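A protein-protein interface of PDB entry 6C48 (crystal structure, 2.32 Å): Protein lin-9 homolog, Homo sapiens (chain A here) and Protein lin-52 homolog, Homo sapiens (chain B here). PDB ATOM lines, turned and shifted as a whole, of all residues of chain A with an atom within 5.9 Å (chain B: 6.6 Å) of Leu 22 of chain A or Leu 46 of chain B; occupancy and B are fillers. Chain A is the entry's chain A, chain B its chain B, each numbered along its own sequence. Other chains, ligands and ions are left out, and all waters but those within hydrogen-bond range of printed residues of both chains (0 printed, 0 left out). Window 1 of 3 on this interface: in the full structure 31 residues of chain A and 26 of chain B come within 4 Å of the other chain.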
ATOM      1  N   ARG A  17     -19.868  36.872 -10.169  1.00  0.00           N
ATOM      2  CA  ARG A  17     -19.575  36.914  -8.743  1.00  0.00           C
ATOM      3  C   ARG A  17     -20.053  35.648  -8.049  1.00  0.00           C
ATOM      4  O   ARG A  17     -19.359  35.119  -7.175  1.00  0.00           O
ATOM      5  CB  ARG A  17     -20.201  38.154  -8.112  1.00  0.00           C
ATOM      6  CG  ARG A  17     -19.525  39.402  -8.587  1.00  0.00           C
ATOM      7  CD  ARG A  17     -20.020  40.679  -7.955  1.00  0.00           C
ATOM      8  NE  ARG A  17     -19.177  41.762  -8.446  1.00  0.00           N
ATOM      9  CZ  ARG A  17     -19.538  43.034  -8.535  1.00  0.00           C
ATOM     10  NH1 ARG A  17     -20.745  43.411  -8.155  1.00  0.00           N
ATOM     11  NH2 ARG A  17     -18.686  43.929  -9.016  1.00  0.00           N
ATOM     12  N   LEU A  18     -21.224  35.142  -8.444  1.00  0.00           N
ATOM     13  CA  LEU A  18     -21.718  33.883  -7.915  1.00  0.00           C
ATOM     14  C   LEU A  18     -20.703  32.771  -8.119  1.00  0.00           C
ATOM     15  O   LEU A  18     -20.312  32.084  -7.165  1.00  0.00           O
ATOM     16  CB  LEU A  18     -23.040  33.522  -8.586  1.00  0.00           C
ATOM     17  CG  LEU A  18     -23.683  32.210  -8.135  1.00  0.00           C
ATOM     18  CD1 LEU A  18     -23.775  32.209  -6.643  1.00  0.00           C
ATOM     19  CD2 LEU A  18     -25.084  32.080  -8.745  1.00  0.00           C
ATOM     20  N   SER A  19     -20.260  32.585  -9.365  1.00  0.00           N
ATOM     21  CA  SER A  19     -19.306  31.518  -9.651  1.00  0.00           C
ATOM     22  C   SER A  19     -18.030  31.660  -8.828  1.00  0.00           C
ATOM     23  O   SER A  19     -17.493  30.666  -8.326  1.00  0.00           O
ATOM     24  CB  SER A  19     -18.969  31.496 -11.138  1.00  0.00           C
ATOM     25  OG  SER A  19     -17.900  30.589 -11.355  1.00  0.00           O
ATOM     26  N   LYS A  20     -17.534  32.890  -8.676  1.00  0.00           N
ATOM     27  CA  LYS A  20     -16.264  33.096  -7.991  1.00  0.00           C
ATOM     28  C   LYS A  20     -16.400  32.854  -6.491  1.00  0.00           C
ATOM     29  O   LYS A  20     -15.502  32.268  -5.868  1.00  0.00           O
ATOM     30  CB  LYS A  20     -15.736  34.502  -8.270  1.00  0.00           C
ATOM     31  CG  LYS A  20     -14.453  34.830  -7.515  1.00  0.00           C
ATOM     32  CD  LYS A  20     -14.014  36.264  -7.749  1.00  0.00           C
ATOM     33  CE  LYS A  20     -12.504  36.355  -7.791  1.00  0.00           C
ATOM     34  NZ  LYS A  20     -12.040  37.737  -7.552  1.00  0.00           N
ATOM     35  N   ILE A  21     -17.500  33.325  -5.892  1.00  0.00           N
ATOM     36  CA  ILE A  21     -17.750  33.074  -4.474  1.00  0.00           C
ATOM     37  C   ILE A  21     -17.833  31.573  -4.204  1.00  0.00           C
ATOM     38  O   ILE A  21     -17.219  31.065  -3.263  1.00  0.00           O
ATOM     39  CB  ILE A  21     -19.019  33.810  -4.001  1.00  0.00           C
ATOM     40  CG1 ILE A  21     -18.779  35.324  -3.996  1.00  0.00           C
ATOM     41  CG2 ILE A  21     -19.431  33.332  -2.591  1.00  0.00           C
ATOM     42  CD1 ILE A  21     -20.038  36.137  -3.849  1.00  0.00           C
ATOM     43  N   LEU A  22     -18.560  30.835  -5.048  1.00  0.00           N
ATOM     44  CA  LEU A  22     -18.705  29.401  -4.819  1.00  0.00           C
ATOM     45  C   LEU A  22     -17.373  28.665  -4.936  1.00  0.00           C
ATOM     46  O   LEU A  22     -17.124  27.705  -4.195  1.00  0.00           O
ATOM     47  CB  LEU A  22     -19.723  28.815  -5.785  1.00  0.00           C
ATOM     48  CG  LEU A  22     -21.109  29.389  -5.536  1.00  0.00           C
ATOM     49  CD1 LEU A  22     -22.143  28.737  -6.461  1.00  0.00           C
ATOM     50  CD2 LEU A  22     -21.476  29.229  -4.066  1.00  0.00           C
ATOM     51  N   MET A  23     -16.514  29.082  -5.873  1.00  0.00           N
ATOM     52  CA  MET A  23     -15.229  28.419  -6.048  1.00  0.00           C
ATOM     53  C   MET A  23     -14.338  28.621  -4.827  1.00  0.00           C
ATOM     54  O   MET A  23     -13.662  27.686  -4.389  1.00  0.00           O
ATOM     55  CB  MET A  23     -14.537  28.919  -7.323  1.00  0.00           C
ATOM     56  CG  MET A  23     -15.164  28.410  -8.657  1.00  0.00           C
ATOM     57  SD  MET A  23     -15.514  26.608  -8.758  1.00  0.00           S
ATOM     58  CE  MET A  23     -17.265  26.588  -8.417  1.00  0.00           C
ATOM     59  N   ILE A  24     -14.337  29.827  -4.254  1.00  0.00           N
ATOM     60  CA  ILE A  24     -13.561  30.069  -3.043  1.00  0.00           C
ATOM     61  C   ILE A  24     -14.159  29.309  -1.867  1.00  0.00           C
ATOM     62  O   ILE A  24     -13.432  28.725  -1.054  1.00  0.00           O
ATOM     63  CB  ILE A  24     -13.478  31.576  -2.748  1.00  0.00           C
ATOM     64  CG1 ILE A  24     -12.859  32.334  -3.920  1.00  0.00           C
ATOM     65  CG2 ILE A  24     -12.681  31.827  -1.494  1.00  0.00           C
ATOM     66  CD1 ILE A  24     -12.768  33.823  -3.665  1.00  0.00           C
ATOM     67  N   LYS A  25     -15.490  29.325  -1.750  1.00  0.00           N
ATOM     68  CA  LYS A  25     -16.160  28.670  -0.631  1.00  0.00           C
ATOM     69  C   LYS A  25     -15.955  27.163  -0.674  1.00  0.00           C
ATOM     70  O   LYS A  25     -15.808  26.522   0.375  1.00  0.00           O
ATOM     71  CB  LYS A  25     -17.649  29.023  -0.636  1.00  0.00           C
ATOM     72  CG  LYS A  25     -18.484  28.310   0.422  1.00  0.00           C
ATOM     73  CD  LYS A  25     -19.894  28.907   0.542  1.00  0.00           C
ATOM     74  CE  LYS A  25     -20.771  28.036   1.449  1.00  0.00           C
ATOM     75  NZ  LYS A  25     -22.050  28.698   1.819  1.00  0.00           N
ATOM     76  N   LYS A  26     -15.936  26.584  -1.880  1.00  0.00           N
ATOM     77  CA  LYS A  26     -15.585  25.171  -2.030  1.00  0.00           C
ATOM     78  C   LYS A  26     -14.192  24.878  -1.471  1.00  0.00           C
ATOM     79  O   LYS A  26     -14.003  23.892  -0.747  1.00  0.00           O
ATOM     80  CB  LYS A  26     -15.698  24.756  -3.493  1.00  0.00           C
ATOM     81  CG  LYS A  26     -15.722  23.254  -3.700  1.00  0.00           C
ATOM     82  CD  LYS A  26     -15.125  22.845  -5.043  1.00  0.00           C
ATOM     83  CE  LYS A  26     -16.188  22.863  -6.141  1.00  0.00           C
ATOM     84  NZ  LYS A  26     -16.679  21.503  -6.525  1.00  0.00           N
ATOM     85  N   GLU A  27     -13.196  25.708  -1.808  1.00  0.00           N
ATOM     86  CA  GLU A  27     -11.855  25.495  -1.255  1.00  0.00           C
ATOM     87  C   GLU A  27     -11.871  25.548   0.266  1.00  0.00           C
ATOM     88  O   GLU A  27     -11.274  24.699   0.935  1.00  0.00           O
ATOM     89  CB  GLU A  27     -10.869  26.540  -1.776  1.00  0.00           C
ATOM     90  CG  GLU A  27     -10.739  26.614  -3.266  1.00  0.00           C
ATOM     91  CD  GLU A  27      -9.508  25.893  -3.765  1.00  0.00           C
ATOM     92  OE1 GLU A  27      -8.979  26.297  -4.832  1.00  0.00           O
ATOM     93  OE2 GLU A  27      -9.077  24.921  -3.090  1.00  0.00           O
ATOM     94  N   ILE A  29     -14.336  24.929   2.343  1.00  0.00           N
ATOM     95  CA  ILE A  29     -15.014  23.788   2.943  1.00  0.00           C
ATOM     96  C   ILE A  29     -14.113  22.556   2.900  1.00  0.00           C
ATOM     97  O   ILE A  29     -14.060  21.775   3.861  1.00  0.00           O
ATOM     98  CB  ILE A  29     -16.380  23.555   2.261  1.00  0.00           C
ATOM     99  CG1 ILE A  29     -17.313  24.726   2.550  1.00  0.00           C
ATOM    100  CG2 ILE A  29     -17.066  22.269   2.776  1.00  0.00           C
ATOM    101  CD1 ILE A  29     -18.418  24.848   1.524  1.00  0.00           C
ATOM    102  N   LEU A  71     -22.406  35.965  -0.837  1.00  0.00           N
ATOM    103  CA  LEU A  71     -23.236  34.995  -1.538  1.00  0.00           C
ATOM    104  C   LEU A  71     -24.692  35.395  -1.438  1.00  0.00           C
ATOM    105  O   LEU A  71     -25.420  35.392  -2.435  1.00  0.00           O
ATOM    106  CB  LEU A  71     -23.027  33.603  -0.941  1.00  0.00           C
ATOM    107  CG  LEU A  71     -23.651  32.459  -1.732  1.00  0.00           C
ATOM    108  CD1 LEU A  71     -23.282  32.601  -3.193  1.00  0.00           C
ATOM    109  CD2 LEU A  71     -23.184  31.115  -1.200  1.00  0.00           C
ATOM    110  N   GLY B  38     -26.891  25.373 -12.519  1.00  0.00           N
ATOM    111  CA  GLY B  38     -25.801  24.623 -11.922  1.00  0.00           C
ATOM    112  C   GLY B  38     -25.159  25.353 -10.758  1.00  0.00           C
ATOM    113  O   GLY B  38     -24.822  24.742  -9.740  1.00  0.00           O
ATOM    114  N   LEU B  39     -24.978  26.673 -10.895  1.00  0.00           N
ATOM    115  CA  LEU B  39     -24.362  27.440  -9.824  1.00  0.00           C
ATOM    116  C   LEU B  39     -25.284  27.521  -8.623  1.00  0.00           C
ATOM    117  O   LEU B  39     -24.820  27.500  -7.476  1.00  0.00           O
ATOM    118  CB  LEU B  39     -23.994  28.839 -10.306  1.00  0.00           C
ATOM    119  CG  LEU B  39     -22.859  28.954 -11.323  1.00  0.00           C
ATOM    120  CD1 LEU B  39     -22.895  30.333 -11.962  1.00  0.00           C
ATOM    121  CD2 LEU B  39     -21.518  28.702 -10.672  1.00  0.00           C
ATOM    122  N   GLN B  40     -26.592  27.629  -8.864  1.00  0.00           N
ATOM    123  CA  GLN B  40     -27.528  27.635  -7.748  1.00  0.00           C
ATOM    124  C   GLN B  40     -27.531  26.285  -7.046  1.00  0.00           C
ATOM    125  O   GLN B  40     -27.476  26.229  -5.817  1.00  0.00           O
ATOM    126  CB  GLN B  40     -28.935  28.009  -8.216  1.00  0.00           C
ATOM    127  CG  GLN B  40     -29.102  29.494  -8.582  1.00  0.00           C
ATOM    128  CD  GLN B  40     -30.386  29.755  -9.367  1.00  0.00           C
ATOM    129  OE1 GLN B  40     -30.829  28.901 -10.129  1.00  0.00           O
ATOM    130  NE2 GLN B  40     -30.985  30.932  -9.182  1.00  0.00           N
ATOM    131  N   ASN B  41     -27.559  25.189  -7.812  1.00  0.00           N
ATOM    132  CA  ASN B  41     -27.477  23.867  -7.208  1.00  0.00           C
ATOM    133  C   ASN B  41     -26.169  23.695  -6.440  1.00  0.00           C
ATOM    134  O   ASN B  41     -26.148  23.101  -5.356  1.00  0.00           O
ATOM    135  CB  ASN B  41     -27.598  22.794  -8.285  1.00  0.00           C
ATOM    136  CG  ASN B  41     -28.919  22.848  -9.016  1.00  0.00           C
ATOM    137  OD1 ASN B  41     -29.947  23.226  -8.445  1.00  0.00           O
ATOM    138  ND2 ASN B  41     -28.901  22.476 -10.294  1.00  0.00           N
ATOM    139  N   LEU B  42     -25.073  24.234  -6.977  1.00  0.00           N
ATOM    140  CA  LEU B  42     -23.796  24.115  -6.297  1.00  0.00           C
ATOM    141  C   LEU B  42     -23.816  24.861  -4.964  1.00  0.00           C
ATOM    142  O   LEU B  42     -23.306  24.359  -3.956  1.00  0.00           O
ATOM    143  CB  LEU B  42     -22.683  24.629  -7.198  1.00  0.00           C
ATOM    144  CG  LEU B  42     -21.324  24.753  -6.527  1.00  0.00           C
ATOM    145  CD1 LEU B  42     -20.801  23.379  -6.129  1.00  0.00           C
ATOM    146  CD2 LEU B  42     -20.363  25.458  -7.437  1.00  0.00           C
ATOM    147  N   ALA B  43     -24.396  26.065  -4.941  1.00  0.00           N
ATOM    148  CA  ALA B  43     -24.551  26.784  -3.685  1.00  0.00           C
ATOM    149  C   ALA B  43     -25.229  25.903  -2.647  1.00  0.00           C
ATOM    150  O   ALA B  43     -24.762  25.783  -1.507  1.00  0.00           O
ATOM    151  CB  ALA B  43     -25.352  28.064  -3.903  1.00  0.00           C
ATOM    152  N   TYR B  44     -26.316  25.242  -3.042  1.00  0.00           N
ATOM    153  CA  TYR B  44     -27.064  24.440  -2.085  1.00  0.00           C
ATOM    154  C   TYR B  44     -26.259  23.239  -1.598  1.00  0.00           C
ATOM    155  O   TYR B  44     -26.258  22.936  -0.399  1.00  0.00           O
ATOM    156  CB  TYR B  44     -28.389  23.997  -2.694  1.00  0.00           C
ATOM    157  CG  TYR B  44     -29.275  23.378  -1.655  1.00  0.00           C
ATOM    158  CD1 TYR B  44     -29.942  24.171  -0.726  1.00  0.00           C
ATOM    159  CD2 TYR B  44     -29.428  21.997  -1.581  1.00  0.00           C
ATOM    160  CE1 TYR B  44     -30.750  23.605   0.247  1.00  0.00           C
ATOM    161  CE2 TYR B  44     -30.235  21.420  -0.618  1.00  0.00           C
ATOM    162  CZ  TYR B  44     -30.895  22.226   0.293  1.00  0.00           C
ATOM    163  OH  TYR B  44     -31.703  21.640   1.251  1.00  0.00           O
ATOM    164  N   GLN B  45     -25.563  22.557  -2.509  1.00  0.00           N
ATOM    165  CA  GLN B  45     -24.791  21.370  -2.158  1.00  0.00           C
ATOM    166  C   GLN B  45     -23.635  21.740  -1.227  1.00  0.00           C
ATOM    167  O   GLN B  45     -23.392  21.075  -0.203  1.00  0.00           O
ATOM    168  CB  GLN B  45     -24.272  20.726  -3.446  1.00  0.00           C
ATOM    169  CG  GLN B  45     -25.331  19.983  -4.323  1.00  0.00           C
ATOM    170  CD  GLN B  45     -26.152  18.899  -3.609  1.00  0.00           C
ATOM    171  OE1 GLN B  45     -27.035  19.194  -2.802  1.00  0.00           O
ATOM    172  NE2 GLN B  45     -25.914  17.643  -3.976  1.00  0.00           N
ATOM    173  N   LEU B  46     -22.910  22.808  -1.574  1.00  0.00           N
ATOM    174  CA  LEU B  46     -21.851  23.316  -0.713  1.00  0.00           C
ATOM    175  C   LEU B  46     -22.395  23.737   0.641  1.00  0.00           C
ATOM    176  O   LEU B  46     -21.745  23.524   1.666  1.00  0.00           O
ATOM    177  CB  LEU B  46     -21.159  24.498  -1.378  1.00  0.00           C
ATOM    178  CG  LEU B  46     -20.192  24.201  -2.506  1.00  0.00           C
ATOM    179  CD1 LEU B  46     -19.641  25.518  -3.001  1.00  0.00           C
ATOM    180  CD2 LEU B  46     -19.081  23.315  -1.997  1.00  0.00           C
ATOM    181  N   GLY B  47     -23.584  24.343   0.662  1.00  0.00           N
ATOM    182  CA  GLY B  47     -24.202  24.723   1.922  1.00  0.00           C
ATOM    183  C   GLY B  47     -24.480  23.541   2.830  1.00  0.00           C
ATOM    184  O   GLY B  47     -24.365  23.651   4.050  1.00  0.00           O
ATOM    185  N   LEU B  48     -24.887  22.406   2.250  1.00  0.00           N
ATOM    186  CA  LEU B  48     -25.044  21.189   3.040  1.00  0.00           C
ATOM    187  C   LEU B  48     -23.703  20.713   3.580  1.00  0.00           C
ATOM    188  O   LEU B  48     -23.602  20.328   4.752  1.00  0.00           O
ATOM    189  CB  LEU B  48     -25.672  20.074   2.209  1.00  0.00           C
ATOM    190  CG  LEU B  48     -27.031  20.180   1.529  1.00  0.00           C
ATOM    191  CD1 LEU B  48     -27.244  18.923   0.693  1.00  0.00           C
ATOM    192  CD2 LEU B  48     -28.138  20.356   2.541  1.00  0.00           C
ATOM    193  N   ASP B  49     -22.675  20.685   2.718  1.00  0.00           N
ATOM    194  CA  ASP B  49     -21.337  20.273   3.144  1.00  0.00           C
ATOM    195  C   ASP B  49     -20.839  21.163   4.268  1.00  0.00           C
ATOM    196  O   ASP B  49     -20.403  20.680   5.319  1.00  0.00           O
ATOM    197  CB  ASP B  49     -20.338  20.341   1.987  1.00  0.00           C
ATOM    198  CG  ASP B  49     -20.596  19.322   0.926  1.00  0.00           C
ATOM    199  OD1 ASP B  49     -21.418  18.416   1.160  1.00  0.00           O
ATOM    200  OD2 ASP B  49     -19.904  19.386  -0.116  1.00  0.00           O
ATOM    201  N   GLU B  50     -20.912  22.476   4.049  1.00  0.00           N
ATOM    202  CA  GLU B  50     -20.454  23.455   5.021  1.00  0.00           C
ATOM    203  C   GLU B  50     -21.137  23.265   6.376  1.00  0.00           C
ATOM    204  O   GLU B  50     -20.475  23.225   7.418  1.00  0.00           O
ATOM    205  CB  GLU B  50     -20.726  24.843   4.459  1.00  0.00           C
ATOM    206  CG  GLU B  50     -20.223  26.011   5.255  1.00  0.00           C
ATOM    207  CD  GLU B  50     -20.873  27.304   4.778  1.00  0.00           C
ATOM    208  OE1 GLU B  50     -22.045  27.256   4.360  1.00  0.00           O
ATOM    209  OE2 GLU B  50     -20.219  28.354   4.796  1.00  0.00           O
ATOM    210  N   SER B  51     -22.465  23.138   6.383  1.00  0.00           N
ATOM    211  CA  SER B  51     -23.159  23.002   7.655  1.00  0.00           C
ATOM    212  C   SER B  51     -22.776  21.708   8.366  1.00  0.00           C
ATOM    213  O   SER B  51     -22.652  21.694   9.601  1.00  0.00           O
ATOM    214  CB  SER B  51     -24.669  23.071   7.442  1.00  0.00           C
ATOM    215  OG  SER B  51     -25.111  21.977   6.660  1.00  0.00           O
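NZ of Lys 25 of chain A is in salt-bridge range of OE1 of Glu 50 of chain B (2.9 Å).
Among the printed residues, pairs that only touch across the chains: Leu 22 of chain A with Leu 39 of chain B (3.1 Å), Met 23 of chain A with Leu 42 of chain B (3.4 Å), Leu 22 of chain A with Leu 46 of chain B (3.5 Å), Ile 29 of chain A with Leu 46 of chain B (3.6 Å), Ser 19 of chain A with Leu 39 of chain B (3.7 Å), Ile 29 of chain A with Glu 50 of chain B (3.7 Å), Leu 18 of chain A with Leu 39 of chain B (3.8 Å), Lys 26 of chain A with Leu 46 of chain B (3.8 Å), Leu 22 of chain A with Leu 42 of chain B (3.8 Å), Leu 22 of chain A with Ala 43 of chain B (3.8 Å) and Ile 29 of chain A with Asp 49 of chain B (3.9 Å).
Of the printed residues of chain B, Leu 18 of chain A touches Leu 39 (3.8 Å). Printed residues of chain B within 4 Å of Ser 19 of chain A: Leu 39 (3.7 Å). Leu 22 of chain A touches just these residues of chain B: Leu 39 (3.1 Å), Leu 42 (3.8 Å), Ala 43 (3.8 Å) and Leu 46 (3.5 Å). Of the printed residues of chain B, Lys 25 of chain A touches Glu 50 (2.9 Å). Printed residues of chain B within 4 Å of Ile 29 of chain A: Leu 46, Asp 49 and Glu 50. Printed residues of chain A within 4 Å of Ala 43 of chain B: Leu 22 (3.8 Å).
Printed residues of chain A that touch a printed residue of chain B: Leu 18, Ser 19, Leu 22, Met 23, Lys 25, Lys 26 and Ile 29. Hydrophobic or aromatic side chains of chain A within 4 Å of the printed part of chain B: Leu 18, Leu 22, Met 23 and Ile 29. Of the 14 printed residues of chain B, 6 touch a printed residue of chain A. Hydrophobic or aromatic side chains of chain B that line the printed part of chain A: Leu 39, Leu 42 and Leu 46. Among the printed residues, Asp or Glu carboxylates within 4 Å of a Lys or Arg side-chain nitrogen of the other chain: Lys 25 of chain A with Glu 50 of chain B.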
